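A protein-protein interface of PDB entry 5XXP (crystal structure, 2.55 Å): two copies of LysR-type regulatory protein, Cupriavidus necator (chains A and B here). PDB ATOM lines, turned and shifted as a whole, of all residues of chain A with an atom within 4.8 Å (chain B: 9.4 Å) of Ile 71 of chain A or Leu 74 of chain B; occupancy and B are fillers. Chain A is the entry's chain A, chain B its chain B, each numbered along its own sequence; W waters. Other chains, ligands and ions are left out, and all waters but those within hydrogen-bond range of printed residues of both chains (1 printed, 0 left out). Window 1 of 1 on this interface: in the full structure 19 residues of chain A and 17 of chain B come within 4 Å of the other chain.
Of the printed residues of chain B, Asp 67 of chain A touches Ser 78 (2.9 Å) and Arg 81 (3.2 Å). Of chain B, only Leu 74 and Arg 81 come within 4 Å of Arg 70 of chain A. Ile 71 of chain A touches just one residue of chain B: Leu 74. Of the printed residues of chain B, Ala 75 of chain A touches Met 1 (3.6 Å) and Ile 71 (3.8 Å). The nearest residue of chain A that does not touch Leu 74 of chain B is Asp 67 of chain A (4.5 Å).
Water W1 bridges the backbone NH (N) of Phe 3 of chain B (3.0 Å) and the backbone NH (N) of Phe 3 of chain A (3.0 Å).
The guanidinium group (NH1) of Arg 81 of chain B lies within salt-bridge range of the side-chain carboxylate (OD2) of Asp 67 of chain A, 3.2 Å away. OG of Ser 78 of chain B sits close to OD2 of Asp 67 of chain A.
Phe 3 of chain B touches its own counterpart, Phe 3 of chain A. Arg 70 of chain A touches Leu 74 of chain B, but with the chains exchanged Leu 74 of chain A does not touch Arg 70 of chain B (4.03 Å). Ile 71 of chain A touches Leu 74 of chain B, and with the chains exchanged Leu 74 of chain A touches Ile 71 of chain B. Ala 75 of chain A touches Ile 71 of chain B, but with the chains exchanged Ile 71 of chain A does not touch Ala 75 of chain B (4.1 Å). Of the 11 pairs that touch across the chains among the printed residues, 4 have their exchanged pair printed and touching as well.
Of the 20 printed residues of chain B, 6 touch a printed residue of chain A. Hydrophobic or aromatic side chains of chain A that line the printed part of chain B: Phe 3, Ile 71, Leu 74 and Ala 75. Among the printed residues, 11 pairs touch across the chains. Among the printed residues, Asp or Glu carboxylates within 4 Å of a Lys or Arg side-chain nitrogen of the other chain: Asp 67 of chain A with Arg 81 of chain B.
Among the printed residues, pairs that only touch across the chains: Phe 3 of chain A with Met 1 of chain B, Ile 71 of chain A with Leu 74 of chain B, Ala 75 of chain A with Met 1 of chain B, Arg 70 of chain A with Arg 81 of chain B, Leu 74 of chain A with Ile 71 of chain B, Leu 74 of chain A with Leu 74 of chain B, Arg 70 of chain A with Leu 74 of chain B, Phe 3 of chain A with Phe 3 of chain B and Ala 75 of chain A with Ile 71 of chain B.
OD1 of Asp 67 of chain A lies within salt-bridge range of NH2 of Arg 70 of chain A, at 3.0 Å. OG of Ser 78 of chain B is in hydrogen-bond range of O of Leu 74 of chain B.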
ATOM      1  N   PHE A   3       9.199  20.318  16.057  1.00  0.00           N
ATOM      2  CA  PHE A   3       8.640  21.593  15.577  1.00  0.00           C
ATOM      3  C   PHE A   3       8.891  21.768  14.098  1.00  0.00           C
ATOM      4  O   PHE A   3       8.024  22.224  13.366  1.00  0.00           O
ATOM      5  CB  PHE A   3       9.112  22.776  16.389  1.00  0.00           C
ATOM      6  CG  PHE A   3       8.310  22.979  17.628  1.00  0.00           C
ATOM      7  CD1 PHE A   3       7.007  23.388  17.544  1.00  0.00           C
ATOM      8  CD2 PHE A   3       8.845  22.708  18.871  1.00  0.00           C
ATOM      9  CE1 PHE A   3       6.244  23.569  18.691  1.00  0.00           C
ATOM     10  CE2 PHE A   3       8.089  22.879  20.030  1.00  0.00           C
ATOM     11  CZ  PHE A   3       6.782  23.309  19.939  1.00  0.00           C
ATOM     12  N   LEU A   6       6.405  20.104  11.828  1.00  0.00           N
ATOM     13  CA  LEU A   6       5.133  20.813  11.756  1.00  0.00           C
ATOM     14  C   LEU A   6       5.175  21.954  10.738  1.00  0.00           C
ATOM     15  O   LEU A   6       4.261  22.058   9.909  1.00  0.00           O
ATOM     16  CB  LEU A   6       4.702  21.312  13.133  1.00  0.00           C
ATOM     17  CG  LEU A   6       4.547  20.206  14.190  1.00  0.00           C
ATOM     18  CD1 LEU A   6       3.801  20.703  15.400  1.00  0.00           C
ATOM     19  CD2 LEU A   6       3.838  18.991  13.635  1.00  0.00           C
ATOM     20  N   ASP A  67      -4.367  21.004  13.537  1.00  0.00           N
ATOM     21  CA  ASP A  67      -3.716  20.979  14.837  1.00  0.00           C
ATOM     22  C   ASP A  67      -2.260  21.463  14.832  1.00  0.00           C
ATOM     23  O   ASP A  67      -1.802  22.074  15.818  1.00  0.00           O
ATOM     24  CB  ASP A  67      -3.855  19.603  15.445  1.00  0.00           C
ATOM     25  CG  ASP A  67      -5.271  19.330  15.913  1.00  0.00           C
ATOM     26  OD1 ASP A  67      -5.886  20.266  16.480  1.00  0.00           O
ATOM     27  OD2 ASP A  67      -5.771  18.198  15.716  1.00  0.00           O
ATOM     28  N   ALA A  68      -1.553  21.213  13.718  1.00  0.00           N
ATOM     29  CA  ALA A  68      -0.224  21.769  13.505  1.00  0.00           C
ATOM     30  C   ALA A  68      -0.195  23.272  13.556  1.00  0.00           C
ATOM     31  O   ALA A  68       0.628  23.858  14.254  1.00  0.00           O
ATOM     32  CB  ALA A  68       0.341  21.286  12.183  1.00  0.00           C
ATOM     33  N   ARG A  69      -1.079  23.919  12.813  1.00  0.00           N
ATOM     34  CA  ARG A  69      -1.223  25.372  12.945  1.00  0.00           C
ATOM     35  C   ARG A  69      -1.425  25.811  14.401  1.00  0.00           C
ATOM     36  O   ARG A  69      -0.768  26.746  14.859  1.00  0.00           O
ATOM     37  CB  ARG A  69      -2.358  25.886  12.073  1.00  0.00           C
ATOM     38  CG  ARG A  69      -2.000  25.968  10.612  1.00  0.00           C
ATOM     39  CD  ARG A  69      -3.237  26.176   9.732  1.00  0.00           C
ATOM     40  NE  ARG A  69      -2.856  26.431   8.337  1.00  0.00           N
ATOM     41  CZ  ARG A  69      -3.505  25.998   7.252  1.00  0.00           C
ATOM     42  NH1 ARG A  69      -3.042  26.291   6.032  1.00  0.00           N
ATOM     43  NH2 ARG A  69      -4.601  25.266   7.347  1.00  0.00           N
ATOM     44  N   ARG A  70      -2.299  25.141  15.134  1.00  0.00           N
ATOM     45  CA  ARG A  70      -2.560  25.538  16.546  1.00  0.00           C
ATOM     46  C   ARG A  70      -1.407  25.297  17.522  1.00  0.00           C
ATOM     47  O   ARG A  70      -1.326  25.943  18.578  1.00  0.00           O
ATOM     48  CB  ARG A  70      -3.763  24.796  17.127  1.00  0.00           C
ATOM     49  CG  ARG A  70      -5.102  25.048  16.442  1.00  0.00           C
ATOM     50  CD  ARG A  70      -6.254  24.769  17.421  1.00  0.00           C
ATOM     51  NE  ARG A  70      -6.578  23.337  17.614  1.00  0.00           N
ATOM     52  CZ  ARG A  70      -7.034  22.800  18.754  1.00  0.00           C
ATOM     53  NH1 ARG A  70      -7.201  23.530  19.841  1.00  0.00           N
ATOM     54  NH2 ARG A  70      -7.313  21.509  18.819  1.00  0.00           N
ATOM     55  N   ILE A  71      -0.537  24.344  17.195  1.00  0.00           N
ATOM     56  CA  ILE A  71       0.599  24.040  18.055  1.00  0.00           C
ATOM     57  C   ILE A  71       1.653  25.118  17.850  1.00  0.00           C
ATOM     58  O   ILE A  71       2.294  25.536  18.811  1.00  0.00           O
ATOM     59  CB  ILE A  71       1.142  22.625  17.756  1.00  0.00           C
ATOM     60  CG1 ILE A  71       0.115  21.582  18.191  1.00  0.00           C
ATOM     61  CG2 ILE A  71       2.433  22.353  18.506  1.00  0.00           C
ATOM     62  CD1 ILE A  71       0.304  20.244  17.517  1.00  0.00           C
ATOM     63  N   LEU A  72       1.812  25.576  16.600  1.00  0.00           N
ATOM     64  CA  LEU A  72       2.721  26.677  16.273  1.00  0.00           C
ATOM     65  C   LEU A  72       2.271  28.026  16.836  1.00  0.00           C
ATOM     66  O   LEU A  72       3.058  28.748  17.506  1.00  0.00           O
ATOM     67  CB  LEU A  72       2.968  26.758  14.758  1.00  0.00           C
ATOM     68  CG  LEU A  72       3.734  25.558  14.136  1.00  0.00           C
ATOM     69  CD1 LEU A  72       4.412  25.908  12.820  1.00  0.00           C
ATOM     70  CD2 LEU A  72       4.781  24.996  15.061  1.00  0.00           C
ATOM     71  N   GLU A  73       1.009  28.353  16.598  1.00  0.00           N
ATOM     72  CA  GLU A  73       0.370  29.471  17.275  1.00  0.00           C
ATOM     73  C   GLU A  73       0.665  29.420  18.795  1.00  0.00           C
ATOM     74  O   GLU A  73       1.159  30.375  19.366  1.00  0.00           O
ATOM     75  CB  GLU A  73      -1.143  29.480  16.985  1.00  0.00           C
ATOM     76  CG  GLU A  73      -1.872  30.780  17.307  1.00  0.00           C
ATOM     77  CD  GLU A  73      -1.725  31.829  16.216  1.00  0.00           C
ATOM     78  OE1 GLU A  73      -2.685  31.977  15.426  1.00  0.00           O
ATOM     79  OE2 GLU A  73      -0.664  32.507  16.141  1.00  0.00           O
ATOM     80  N   LEU A  74       0.397  28.296  19.434  1.00  0.00           N
ATOM     81  CA  LEU A  74       0.515  28.222  20.894  1.00  0.00           C
ATOM     82  C   LEU A  74       1.977  28.322  21.357  1.00  0.00           C
ATOM     83  O   LEU A  74       2.290  28.889  22.402  1.00  0.00           O
ATOM     84  CB  LEU A  74      -0.120  26.933  21.371  1.00  0.00           C
ATOM     85  CG  LEU A  74      -0.179  26.614  22.851  1.00  0.00           C
ATOM     86  CD1 LEU A  74      -0.976  27.652  23.607  1.00  0.00           C
ATOM     87  CD2 LEU A  74      -0.832  25.253  23.039  1.00  0.00           C
ATOM     88  N   ALA A  75       2.885  27.765  20.582  1.00  0.00           N
ATOM     89  CA  ALA A  75       4.280  27.853  20.949  1.00  0.00           C
ATOM     90  C   ALA A  75       4.700  29.306  20.874  1.00  0.00           C
ATOM     91  O   ALA A  75       5.318  29.800  21.801  1.00  0.00           O
ATOM     92  CB  ALA A  75       5.142  27.012  20.018  1.00  0.00           C
ATOM     93  N   MET B   1      13.115  26.545  19.992  1.00  0.00           N
ATOM     94  CA  MET B   1      12.229  25.795  20.915  1.00  0.00           C
ATOM     95  C   MET B   1      12.069  24.418  20.329  1.00  0.00           C
ATOM     96  O   MET B   1      11.771  24.266  19.139  1.00  0.00           O
ATOM     97  CB  MET B   1      10.864  26.471  21.053  1.00  0.00           C
ATOM     98  CG  MET B   1      10.096  26.065  22.293  1.00  0.00           C
ATOM     99  SD  MET B   1       8.360  26.551  22.174  1.00  0.00           S
ATOM    100  CE  MET B   1       8.449  28.239  22.759  1.00  0.00           C
ATOM    101  N   PHE B   3      10.510  20.266  21.276  1.00  0.00           N
ATOM    102  CA  PHE B   3       9.699  19.438  22.163  1.00  0.00           C
ATOM    103  C   PHE B   3      10.463  18.849  23.313  1.00  0.00           C
ATOM    104  O   PHE B   3       9.936  18.767  24.407  1.00  0.00           O
ATOM    105  CB  PHE B   3       9.031  18.310  21.409  1.00  0.00           C
ATOM    106  CG  PHE B   3       7.814  18.740  20.698  1.00  0.00           C
ATOM    107  CD1 PHE B   3       6.702  19.068  21.400  1.00  0.00           C
ATOM    108  CD2 PHE B   3       7.802  18.856  19.337  1.00  0.00           C
ATOM    109  CE1 PHE B   3       5.560  19.487  20.756  1.00  0.00           C
ATOM    110  CE2 PHE B   3       6.667  19.276  18.672  1.00  0.00           C
ATOM    111  CZ  PHE B   3       5.536  19.594  19.384  1.00  0.00           C
ATOM    112  N   LEU B   6      10.808  21.196  26.210  1.00  0.00           N
ATOM    113  CA  LEU B   6       9.556  21.307  26.927  1.00  0.00           C
ATOM    114  C   LEU B   6       9.450  20.177  27.925  1.00  0.00           C
ATOM    115  O   LEU B   6       9.176  20.454  29.060  1.00  0.00           O
ATOM    116  CB  LEU B   6       8.359  21.367  25.978  1.00  0.00           C
ATOM    117  CG  LEU B   6       8.245  22.613  25.068  1.00  0.00           C
ATOM    118  CD1 LEU B   6       6.827  22.961  24.719  1.00  0.00           C
ATOM    119  CD2 LEU B   6       8.886  23.829  25.673  1.00  0.00           C
ATOM    120  N   GLU B  66       3.179  26.365  32.466  1.00  0.00           N
ATOM    121  CA  GLU B  66       1.778  26.074  32.172  1.00  0.00           C
ATOM    122  C   GLU B  66       1.585  25.859  30.664  1.00  0.00           C
ATOM    123  O   GLU B  66       0.843  24.961  30.254  1.00  0.00           O
ATOM    124  CB  GLU B  66       0.840  27.183  32.695  1.00  0.00           C
ATOM    125  CG  GLU B  66       0.694  27.340  34.223  1.00  0.00           C
ATOM    126  CD  GLU B  66       0.944  26.072  35.078  1.00  0.00           C
ATOM    127  OE1 GLU B  66       0.448  24.945  34.762  1.00  0.00           O
ATOM    128  OE2 GLU B  66       1.648  26.215  36.116  1.00  0.00           O
ATOM    129  N   ASP B  67       2.263  26.658  29.853  1.00  0.00           N
ATOM    130  CA  ASP B  67       2.101  26.604  28.391  1.00  0.00           C
ATOM    131  C   ASP B  67       2.846  25.443  27.768  1.00  0.00           C
ATOM    132  O   ASP B  67       2.388  24.836  26.791  1.00  0.00           O
ATOM    133  CB  ASP B  67       2.604  27.894  27.765  1.00  0.00           C
ATOM    134  CG  ASP B  67       1.658  29.059  28.011  1.00  0.00           C
ATOM    135  OD1 ASP B  67       0.430  28.836  27.935  1.00  0.00           O
ATOM    136  OD2 ASP B  67       2.128  30.185  28.291  1.00  0.00           O
ATOM    137  N   ALA B  68       4.002  25.147  28.346  1.00  0.00           N
ATOM    138  CA  ALA B  68       4.668  23.886  28.157  1.00  0.00           C
ATOM    139  C   ALA B  68       3.716  22.716  28.281  1.00  0.00           C
ATOM    140  O   ALA B  68       3.596  21.912  27.360  1.00  0.00           O
ATOM    141  CB  ALA B  68       5.788  23.753  29.162  1.00  0.00           C
ATOM    142  N   ARG B  69       3.024  22.614  29.402  1.00  0.00           N
ATOM    143  CA  ARG B  69       2.040  21.540  29.566  1.00  0.00           C
ATOM    144  C   ARG B  69       0.927  21.559  28.492  1.00  0.00           C
ATOM    145  O   ARG B  69       0.565  20.525  27.925  1.00  0.00           O
ATOM    146  CB  ARG B  69       1.469  21.561  30.964  1.00  0.00           C
ATOM    147  CG  ARG B  69       2.437  21.068  32.019  1.00  0.00           C
ATOM    148  CD  ARG B  69       1.939  21.382  33.431  1.00  0.00           C
ATOM    149  NE  ARG B  69       2.662  20.610  34.440  1.00  0.00           N
ATOM    150  CZ  ARG B  69       2.921  21.010  35.684  1.00  0.00           C
ATOM    151  NH1 ARG B  69       2.524  22.197  36.127  1.00  0.00           N
ATOM    152  NH2 ARG B  69       3.599  20.208  36.497  1.00  0.00           N
ATOM    153  N   ARG B  70       0.401  22.726  28.196  1.00  0.00           N
ATOM    154  CA  ARG B  70      -0.599  22.852  27.122  1.00  0.00           C
ATOM    155  C   ARG B  70      -0.080  22.334  25.791  1.00  0.00           C
ATOM    156  O   ARG B  70      -0.792  21.645  25.071  1.00  0.00           O
ATOM    157  CB  ARG B  70      -1.054  24.318  26.952  1.00  0.00           C
ATOM    158  CG  ARG B  70      -2.064  24.796  27.995  1.00  0.00           C
ATOM    159  CD  ARG B  70      -2.524  26.249  27.818  1.00  0.00           C
ATOM    160  NE  ARG B  70      -2.048  27.075  28.946  1.00  0.00           N
ATOM    161  CZ  ARG B  70      -2.775  27.501  29.985  1.00  0.00           C
ATOM    162  NH1 ARG B  70      -4.067  27.229  30.098  1.00  0.00           N
ATOM    163  NH2 ARG B  70      -2.195  28.228  30.928  1.00  0.00           N
ATOM    164  N   ILE B  71       1.158  22.669  25.446  1.00  0.00           N
ATOM    165  CA  ILE B  71       1.660  22.366  24.113  1.00  0.00           C
ATOM    166  C   ILE B  71       1.807  20.867  23.960  1.00  0.00           C
ATOM    167  O   ILE B  71       1.458  20.302  22.934  1.00  0.00           O
ATOM    168  CB  ILE B  71       2.998  23.084  23.852  1.00  0.00           C
ATOM    169  CG1 ILE B  71       2.790  24.593  23.727  1.00  0.00           C
ATOM    170  CG2 ILE B  71       3.620  22.597  22.569  1.00  0.00           C
ATOM    171  CD1 ILE B  71       4.075  25.410  23.854  1.00  0.00           C
ATOM    172  N   LEU B  72       2.315  20.209  24.997  1.00  0.00           N
ATOM    173  CA  LEU B  72       2.599  18.797  24.900  1.00  0.00           C
ATOM    174  C   LEU B  72       1.317  17.968  24.848  1.00  0.00           C
ATOM    175  O   LEU B  72       1.151  17.077  23.996  1.00  0.00           O
ATOM    176  CB  LEU B  72       3.473  18.350  26.062  1.00  0.00           C
ATOM    177  CG  LEU B  72       4.939  18.788  26.049  1.00  0.00           C
ATOM    178  CD1 LEU B  72       5.635  18.060  27.186  1.00  0.00           C
ATOM    179  CD2 LEU B  72       5.605  18.467  24.732  1.00  0.00           C
ATOM    180  N   GLU B  73       0.423  18.275  25.770  1.00  0.00           N
ATOM    181  CA  GLU B  73      -0.933  17.776  25.747  1.00  0.00           C
ATOM    182  C   GLU B  73      -1.563  17.947  24.357  1.00  0.00           C
ATOM    183  O   GLU B  73      -2.101  16.983  23.776  1.00  0.00           O
ATOM    184  CB  GLU B  73      -1.766  18.526  26.789  1.00  0.00           C
ATOM    185  CG  GLU B  73      -3.148  17.938  27.040  1.00  0.00           C
ATOM    186  CD  GLU B  73      -3.893  18.685  28.131  1.00  0.00           C
ATOM    187  OE1 GLU B  73      -5.143  18.736  28.052  1.00  0.00           O
ATOM    188  OE2 GLU B  73      -3.220  19.214  29.062  1.00  0.00           O
ATOM    189  N   LEU B  74      -1.492  19.159  23.814  1.00  0.00           N
ATOM    190  CA  LEU B  74      -2.150  19.417  22.528  1.00  0.00           C
ATOM    191  C   LEU B  74      -1.486  18.578  21.453  1.00  0.00           C
ATOM    192  O   LEU B  74      -2.147  18.077  20.564  1.00  0.00           O
ATOM    193  CB  LEU B  74      -2.133  20.891  22.184  1.00  0.00           C
ATOM    194  CG  LEU B  74      -2.501  21.297  20.756  1.00  0.00           C
ATOM    195  CD1 LEU B  74      -3.953  21.019  20.428  1.00  0.00           C
ATOM    196  CD2 LEU B  74      -2.173  22.767  20.570  1.00  0.00           C
ATOM    197  N   ALA B  75      -0.172  18.410  21.565  1.00  0.00           N
ATOM    198  CA  ALA B  75       0.567  17.597  20.622  1.00  0.00           C
ATOM    199  C   ALA B  75       0.177  16.141  20.728  1.00  0.00           C
ATOM    200  O   ALA B  75       0.134  15.451  19.720  1.00  0.00           O
ATOM    201  CB  ALA B  75       2.061  17.764  20.845  1.00  0.00           C
ATOM    202  N   GLY B  76      -0.087  15.676  21.951  1.00  0.00           N
ATOM    203  CA  GLY B  76      -0.477  14.280  22.185  1.00  0.00           C
ATOM    204  C   GLY B  76      -1.815  13.995  21.542  1.00  0.00           C
ATOM    205  O   GLY B  76      -1.943  13.123  20.679  1.00  0.00           O
ATOM    206  N   ARG B  77      -2.813  14.770  21.947  1.00  0.00           N
ATOM    207  CA  ARG B  77      -4.169  14.653  21.399  1.00  0.00           C
ATOM    208  C   ARG B  77      -4.208  14.796  19.865  1.00  0.00           C
ATOM    209  O   ARG B  77      -4.962  14.083  19.193  1.00  0.00           O
ATOM    210  CB  ARG B  77      -5.108  15.678  22.059  1.00  0.00           C
ATOM    211  CG  ARG B  77      -5.391  15.432  23.547  1.00  0.00           C
ATOM    212  CD  ARG B  77      -6.274  14.213  23.811  1.00  0.00           C
ATOM    213  NE  ARG B  77      -7.289  14.094  22.764  1.00  0.00           N
ATOM    214  CZ  ARG B  77      -7.783  12.957  22.267  1.00  0.00           C
ATOM    215  NH1 ARG B  77      -8.694  13.031  21.302  1.00  0.00           N
ATOM    216  NH2 ARG B  77      -7.393  11.763  22.714  1.00  0.00           N
ATOM    217  N   SER B  78      -3.406  15.690  19.298  1.00  0.00           N
ATOM    218  CA  SER B  78      -3.387  15.829  17.836  1.00  0.00           C
ATOM    219  C   SER B  78      -2.941  14.585  17.078  1.00  0.00           C
ATOM    220  O   SER B  78      -3.434  14.320  15.971  1.00  0.00           O
ATOM    221  CB  SER B  78      -2.554  17.022  17.425  1.00  0.00           C
ATOM    222  OG  SER B  78      -3.183  18.210  17.920  1.00  0.00           O
ATOM    223  N   GLY B  79      -2.031  13.816  17.673  1.00  0.00           N
ATOM    224  CA  GLY B  79      -1.743  12.482  17.171  1.00  0.00           C
ATOM    225  C   GLY B  79      -2.962  11.594  17.159  1.00  0.00           C
ATOM    226  O   GLY B  79      -3.307  11.010  16.145  1.00  0.00           O
ATOM    227  N   ASP B  80      -3.622  11.518  18.308  1.00  0.00           N
ATOM    228  CA  ASP B  80      -4.763  10.620  18.520  1.00  0.00           C
ATOM    229  C   ASP B  80      -5.849  10.908  17.492  1.00  0.00           C
ATOM    230  O   ASP B  80      -6.482   9.993  16.949  1.00  0.00           O
ATOM    231  CB  ASP B  80      -5.341  10.790  19.936  1.00  0.00           C
ATOM    232  CG  ASP B  80      -4.374  10.350  21.061  1.00  0.00           C
ATOM    233  OD1 ASP B  80      -3.575   9.400  20.851  1.00  0.00           O
ATOM    234  OD2 ASP B  80      -4.444  10.943  22.182  1.00  0.00           O
ATOM    235  N   ARG B  81      -6.068  12.184  17.229  1.00  0.00           N
ATOM    236  CA  ARG B  81      -7.093  12.606  16.266  1.00  0.00           C
ATOM    237  C   ARG B  81      -6.780  12.135  14.892  1.00  0.00           C
ATOM    238  O   ARG B  81      -7.659  11.650  14.167  1.00  0.00           O
ATOM    239  CB  ARG B  81      -7.212  14.122  16.200  1.00  0.00           C
ATOM    240  CG  ARG B  81      -8.345  14.644  17.036  1.00  0.00           C
ATOM    241  CD  ARG B  81      -8.339  16.150  17.103  1.00  0.00           C
ATOM    242  NE  ARG B  81      -8.602  16.548  18.481  1.00  0.00           N
ATOM    243  CZ  ARG B  81      -7.845  17.347  19.225  1.00  0.00           C
ATOM    244  NH1 ARG B  81      -6.731  17.896  18.747  1.00  0.00           N
ATOM    245  NH2 ARG B  81      -8.235  17.613  20.463  1.00  0.00           N
ATOM    246  N   SER B  82      -5.521  12.303  14.517  1.00  0.00           N
ATOM    247  CA  SER B  82      -5.134  12.116  13.132  1.00  0.00           C
ATOM    248  C   SER B  82      -5.252  10.638  12.806  1.00  0.00           C
ATOM    249  O   SER B  82      -5.722  10.290  11.744  1.00  0.00           O
ATOM    250  CB  SER B  82      -3.726  12.650  12.879  1.00  0.00           C
ATOM    251  OG  SER B  82      -3.452  12.649  11.497  1.00  0.00           O
HETATM  252  O   HOH W   1      11.076  19.895  18.393  1.00  0.00           O
